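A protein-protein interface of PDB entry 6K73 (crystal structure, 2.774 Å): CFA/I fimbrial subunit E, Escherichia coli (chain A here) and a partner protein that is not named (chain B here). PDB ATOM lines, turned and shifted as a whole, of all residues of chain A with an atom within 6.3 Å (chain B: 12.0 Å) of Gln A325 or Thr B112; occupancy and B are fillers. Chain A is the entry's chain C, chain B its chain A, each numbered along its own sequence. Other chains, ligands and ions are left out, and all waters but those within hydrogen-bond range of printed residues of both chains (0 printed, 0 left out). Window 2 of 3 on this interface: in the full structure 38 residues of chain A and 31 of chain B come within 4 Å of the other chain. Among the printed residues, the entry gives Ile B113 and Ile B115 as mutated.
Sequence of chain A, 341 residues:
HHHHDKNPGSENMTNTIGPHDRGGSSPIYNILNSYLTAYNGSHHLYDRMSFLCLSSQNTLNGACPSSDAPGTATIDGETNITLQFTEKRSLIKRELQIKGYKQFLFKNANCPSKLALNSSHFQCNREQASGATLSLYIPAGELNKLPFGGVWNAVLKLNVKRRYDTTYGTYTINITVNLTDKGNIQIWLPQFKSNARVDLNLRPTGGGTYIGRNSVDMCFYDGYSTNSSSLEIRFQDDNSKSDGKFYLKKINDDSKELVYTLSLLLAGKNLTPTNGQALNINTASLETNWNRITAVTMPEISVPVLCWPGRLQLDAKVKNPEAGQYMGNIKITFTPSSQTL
N of Glu B114 sits at hydrogen-bond distance from O of Tyr A326. OD2 of Asp A199 lies close to O of Ile B113. The backbone carbonyl oxygen (O) of Thr B112 sits at hydrogen-bond distance from the backbone NH (N) of Tyr A326, at 2.7 Å.
Of the printed residues of chain B, Asp A199 touches Ile B113 (2.8 Å). No residue of chain B comes within 4 Å of Lys A250. Ile A251 touches none of the printed residues of chain B. Of chain B, only Leu B111 and Thr B112 come within 4 Å of Gly A324. Gln A325 touches just one residue of chain B: Thr B112. Printed residues of chain B within 4 Å of Tyr A326: Thr B112 (2.7 Å), Ile B113 (3.4 Å) and Glu B114 (3.0 Å). Met A327 touches just one residue of chain B: Glu B114. Of chain A, only Gly A324 (3.9 Å), Gln A325 (3.0 Å) and Tyr A326 (2.7 Å) come within 4 Å of Thr B112. Printed residues of chain A within 4 Å of Ile B113: Asp A199 and Tyr A326. Ile B115 touches none of the printed residues of chain A. The nearest residue of chain A that does not touch Thr B112 is Asp A199 (4.1 Å).
Ala A323 touches Leu B111 (CA to CD1, 3.4 Å). Gly A324 touches Leu B111 (O to CG, 3.4 Å). Thr B112 touches Gly A324. Thr B112 touches Gln A325 (O to CA, 3.0 Å). CA of Ile B113 touches O of Tyr A326, 3.4 Å away. Met A327 touches Glu B114.
Printed residues of chain B that touch a printed residue of chain A: Leu B111, Thr B112, Ile B113 and Glu B114. Hydrophobic or aromatic side chains of chain A that line the printed part of chain B: Tyr A326 and Met A327. Among the printed residues, no Asp or Glu carboxylate lies within 4 Å of a Lys or Arg side-chain nitrogen of the other chain.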
ATOM      1  N   ASP A 199     -30.265  10.182 -20.865  1.00  0.00           N
ATOM      2  CA  ASP A 199     -29.408  11.211 -21.430  1.00  0.00           C
ATOM      3  C   ASP A 199     -29.052  12.201 -20.330  1.00  0.00           C
ATOM      4  O   ASP A 199     -29.938  12.675 -19.609  1.00  0.00           O
ATOM      5  CB  ASP A 199     -30.107  11.927 -22.589  1.00  0.00           C
ATOM      6  CG  ASP A 199     -29.137  12.460 -23.628  1.00  0.00           C
ATOM      7  OD1 ASP A 199     -28.270  13.284 -23.278  1.00  0.00           O
ATOM      8  OD2 ASP A 199     -29.228  12.033 -24.800  1.00  0.00           O
ATOM      9  N   LEU A 200     -27.761  12.479 -20.180  1.00  0.00           N
ATOM     10  CA  LEU A 200     -27.336  13.653 -19.429  1.00  0.00           C
ATOM     11  C   LEU A 200     -27.638  14.879 -20.278  1.00  0.00           C
ATOM     12  O   LEU A 200     -27.022  15.076 -21.330  1.00  0.00           O
ATOM     13  CB  LEU A 200     -25.853  13.571 -19.091  1.00  0.00           C
ATOM     14  CG  LEU A 200     -25.442  12.525 -18.055  1.00  0.00           C
ATOM     15  CD1 LEU A 200     -23.936  12.541 -17.832  1.00  0.00           C
ATOM     16  CD2 LEU A 200     -26.184  12.756 -16.748  1.00  0.00           C
ATOM     17  N   LYS A 249     -16.849   7.014 -23.907  1.00  0.00           N
ATOM     18  CA  LYS A 249     -15.929   7.046 -25.035  1.00  0.00           C
ATOM     19  C   LYS A 249     -16.727   7.477 -26.252  1.00  0.00           C
ATOM     20  O   LYS A 249     -17.867   7.030 -26.425  1.00  0.00           O
ATOM     21  CB  LYS A 249     -15.345   5.639 -25.296  1.00  0.00           C
ATOM     22  CG  LYS A 249     -14.195   5.175 -24.413  1.00  0.00           C
ATOM     23  CD  LYS A 249     -14.637   4.494 -23.120  1.00  0.00           C
ATOM     24  CE  LYS A 249     -13.439   4.069 -22.279  1.00  0.00           C
ATOM     25  NZ  LYS A 249     -13.659   4.191 -20.816  1.00  0.00           N
ATOM     26  N   LYS A 250     -16.180   8.351 -27.093  1.00  0.00           N
ATOM     27  CA  LYS A 250     -16.959   8.698 -28.250  1.00  0.00           C
ATOM     28  C   LYS A 250     -17.171   7.477 -29.003  1.00  0.00           C
ATOM     29  O   LYS A 250     -16.266   6.728 -29.205  1.00  0.00           O
ATOM     30  CB  LYS A 250     -16.248   9.648 -29.180  1.00  0.00           C
ATOM     31  CG  LYS A 250     -17.120   9.967 -30.383  1.00  0.00           C
ATOM     32  CD  LYS A 250     -16.346  10.428 -31.603  1.00  0.00           C
ATOM     33  CE  LYS A 250     -17.169  10.221 -32.869  1.00  0.00           C
ATOM     34  NZ  LYS A 250     -16.678  11.003 -34.039  1.00  0.00           N
ATOM     35  N   ILE A 251     -18.380   7.283 -29.473  1.00  0.00           N
ATOM     36  CA  ILE A 251     -18.680   6.119 -30.257  1.00  0.00           C
ATOM     37  C   ILE A 251     -17.876   6.360 -31.501  1.00  0.00           C
ATOM     38  O   ILE A 251     -17.887   7.469 -32.005  1.00  0.00           O
ATOM     39  CB  ILE A 251     -20.154   6.094 -30.598  1.00  0.00           C
ATOM     40  CG1 ILE A 251     -20.495   4.889 -31.437  1.00  0.00           C
ATOM     41  CG2 ILE A 251     -20.536   7.339 -31.350  1.00  0.00           C
ATOM     42  CD1 ILE A 251     -21.921   4.913 -31.926  1.00  0.00           C
ATOM     43  N   ASN A 252     -17.164   5.355 -31.964  1.00  0.00           N
ATOM     44  CA  ASN A 252     -16.335   5.487 -33.140  1.00  0.00           C
ATOM     45  C   ASN A 252     -15.000   6.126 -32.838  1.00  0.00           C
ATOM     46  O   ASN A 252     -14.197   6.270 -33.725  1.00  0.00           O
ATOM     47  CB  ASN A 252     -17.049   6.247 -34.250  1.00  0.00           C
ATOM     48  CG  ASN A 252     -18.029   5.382 -35.002  1.00  0.00           C
ATOM     49  OD1 ASN A 252     -17.733   4.238 -35.351  1.00  0.00           O
ATOM     50  ND2 ASN A 252     -19.201   5.930 -35.268  1.00  0.00           N
ATOM     51  N   ALA A 323     -17.613  17.603 -30.241  1.00  0.00           N
ATOM     52  CA  ALA A 323     -18.967  17.259 -30.553  1.00  0.00           C
ATOM     53  C   ALA A 323     -19.051  15.876 -31.073  1.00  0.00           C
ATOM     54  O   ALA A 323     -18.048  15.297 -31.407  1.00  0.00           O
ATOM     55  CB  ALA A 323     -19.521  18.233 -31.561  1.00  0.00           C
ATOM     56  N   GLY A 324     -20.266  15.357 -31.120  1.00  0.00           N
ATOM     57  CA  GLY A 324     -20.557  14.007 -31.565  1.00  0.00           C
ATOM     58  C   GLY A 324     -21.033  13.254 -30.349  1.00  0.00           C
ATOM     59  O   GLY A 324     -20.666  13.603 -29.252  1.00  0.00           O
ATOM     60  N   GLN A 325     -21.844  12.226 -30.525  1.00  0.00           N
ATOM     61  CA  GLN A 325     -22.364  11.503 -29.370  1.00  0.00           C
ATOM     62  C   GLN A 325     -21.397  10.613 -28.605  1.00  0.00           C
ATOM     63  O   GLN A 325     -20.346  10.240 -29.081  1.00  0.00           O
ATOM     64  CB  GLN A 325     -23.658  10.762 -29.712  1.00  0.00           C
ATOM     65  CG  GLN A 325     -23.495   9.394 -30.324  1.00  0.00           C
ATOM     66  CD  GLN A 325     -23.755   9.407 -31.796  1.00  0.00           C
ATOM     67  OE1 GLN A 325     -22.962   8.919 -32.579  1.00  0.00           O
ATOM     68  NE2 GLN A 325     -24.867   9.970 -32.183  1.00  0.00           N
ATOM     69  N   TYR A 326     -21.765  10.316 -27.378  1.00  0.00           N
ATOM     70  CA  TYR A 326     -20.972   9.485 -26.547  1.00  0.00           C
ATOM     71  C   TYR A 326     -21.937   8.529 -25.971  1.00  0.00           C
ATOM     72  O   TYR A 326     -23.097   8.803 -25.918  1.00  0.00           O
ATOM     73  CB  TYR A 326     -20.349  10.306 -25.465  1.00  0.00           C
ATOM     74  CG  TYR A 326     -19.215  11.105 -25.957  1.00  0.00           C
ATOM     75  CD1 TYR A 326     -19.325  11.851 -27.090  1.00  0.00           C
ATOM     76  CD2 TYR A 326     -18.023  11.121 -25.294  1.00  0.00           C
ATOM     77  CE1 TYR A 326     -18.269  12.599 -27.550  1.00  0.00           C
ATOM     78  CE2 TYR A 326     -16.971  11.870 -25.750  1.00  0.00           C
ATOM     79  CZ  TYR A 326     -17.099  12.593 -26.886  1.00  0.00           C
ATOM     80  OH  TYR A 326     -16.055  13.332 -27.344  1.00  0.00           O
ATOM     81  N   MET A 327     -21.461   7.385 -25.556  1.00  0.00           N
ATOM     82  CA  MET A 327     -22.320   6.398 -24.979  1.00  0.00           C
ATOM     83  C   MET A 327     -21.629   5.744 -23.824  1.00  0.00           C
ATOM     84  O   MET A 327     -20.436   5.725 -23.779  1.00  0.00           O
ATOM     85  CB  MET A 327     -22.667   5.357 -26.013  1.00  0.00           C
ATOM     86  CG  MET A 327     -23.770   5.748 -26.968  1.00  0.00           C
ATOM     87  SD  MET A 327     -24.098   4.445 -28.170  1.00  0.00           S
ATOM     88  CE  MET A 327     -25.275   5.238 -29.254  1.00  0.00           C
ATOM     89  N   LEU B 111     -23.889  17.288 -30.103  1.00  0.00           N
ATOM     90  CA  LEU B 111     -23.238  16.320 -29.225  1.00  0.00           C
ATOM     91  C   LEU B 111     -24.221  15.793 -28.219  1.00  0.00           C
ATOM     92  O   LEU B 111     -24.907  16.550 -27.563  1.00  0.00           O
ATOM     93  CB  LEU B 111     -22.035  16.951 -28.547  1.00  0.00           C
ATOM     94  CG  LEU B 111     -21.367  16.346 -27.325  1.00  0.00           C
ATOM     95  CD1 LEU B 111     -19.891  16.689 -27.362  1.00  0.00           C
ATOM     96  CD2 LEU B 111     -22.004  16.896 -26.066  1.00  0.00           C
ATOM     97  N   THR B 112     -24.287  14.482 -28.107  1.00  0.00           N
ATOM     98  CA  THR B 112     -25.215  13.855 -27.214  1.00  0.00           C
ATOM     99  C   THR B 112     -24.580  12.768 -26.431  1.00  0.00           C
ATOM    100  O   THR B 112     -23.534  12.311 -26.774  1.00  0.00           O
ATOM    101  CB  THR B 112     -26.348  13.247 -27.997  1.00  0.00           C
ATOM    102  OG1 THR B 112     -25.927  13.175 -29.348  1.00  0.00           O
ATOM    103  CG2 THR B 112     -27.553  14.127 -27.923  1.00  0.00           C
ATOM    104  N   ILE B 113     -25.245  12.371 -25.361  1.00  0.00           N
ATOM    105  CA  ILE B 113     -24.775  11.353 -24.466  1.00  0.00           C
ATOM    106  C   ILE B 113     -25.842  10.342 -24.114  1.00  0.00           C
ATOM    107  O   ILE B 113     -26.899  10.724 -23.700  1.00  0.00           O
ATOM    108  CB  ILE B 113     -24.361  12.060 -23.195  1.00  0.00           C
ATOM    109  CG1 ILE B 113     -23.152  12.891 -23.494  1.00  0.00           C
ATOM    110  CG2 ILE B 113     -23.991  11.102 -22.097  1.00  0.00           C
ATOM    111  CD1 ILE B 113     -22.634  13.608 -22.286  1.00  0.00           C
ATOM    112  N   GLU B 114     -25.558   9.054 -24.262  1.00  0.00           N
ATOM    113  CA  GLU B 114     -26.527   8.028 -23.907  1.00  0.00           C
ATOM    114  C   GLU B 114     -25.903   7.052 -22.953  1.00  0.00           C
ATOM    115  O   GLU B 114     -24.869   6.505 -23.207  1.00  0.00           O
ATOM    116  CB  GLU B 114     -27.108   7.310 -25.110  1.00  0.00           C
ATOM    117  CG  GLU B 114     -28.403   7.911 -25.627  1.00  0.00           C
ATOM    118  CD  GLU B 114     -29.647   7.342 -24.975  1.00  0.00           C
ATOM    119  OE1 GLU B 114     -30.701   8.003 -24.979  1.00  0.00           O
ATOM    120  OE2 GLU B 114     -29.569   6.224 -24.463  1.00  0.00           O
ATOM    121  N   ILE B 115     -26.563   6.848 -21.829  1.00  0.00           N
ATOM    122  CA  ILE B 115     -26.034   5.961 -20.794  1.00  0.00           C
ATOM    123  C   ILE B 115     -27.062   4.865 -20.546  1.00  0.00           C
ATOM    124  O   ILE B 115     -28.041   5.067 -19.816  1.00  0.00           O
ATOM    125  CB  ILE B 115     -25.687   6.708 -19.502  1.00  0.00           C
ATOM    126  CG1 ILE B 115     -24.668   7.809 -19.796  1.00  0.00           C
ATOM    127  CG2 ILE B 115     -25.113   5.741 -18.471  1.00  0.00           C
ATOM    128  CD1 ILE B 115     -24.175   8.565 -18.566  1.00  0.00           C
ATOM    129  N   SER B 116     -26.832   3.692 -21.136  1.00  0.00           N
ATOM    130  CA  SER B 116     -27.691   2.537 -20.907  1.00  0.00           C
ATOM    131  C   SER B 116     -27.365   1.913 -19.556  1.00  0.00           C
ATOM    132  O   SER B 116     -26.198   1.667 -19.239  1.00  0.00           O
ATOM    133  CB  SER B 116     -27.534   1.506 -22.024  1.00  0.00           C
ATOM    134  OG  SER B 116     -26.374   1.754 -22.798  1.00  0.00           O
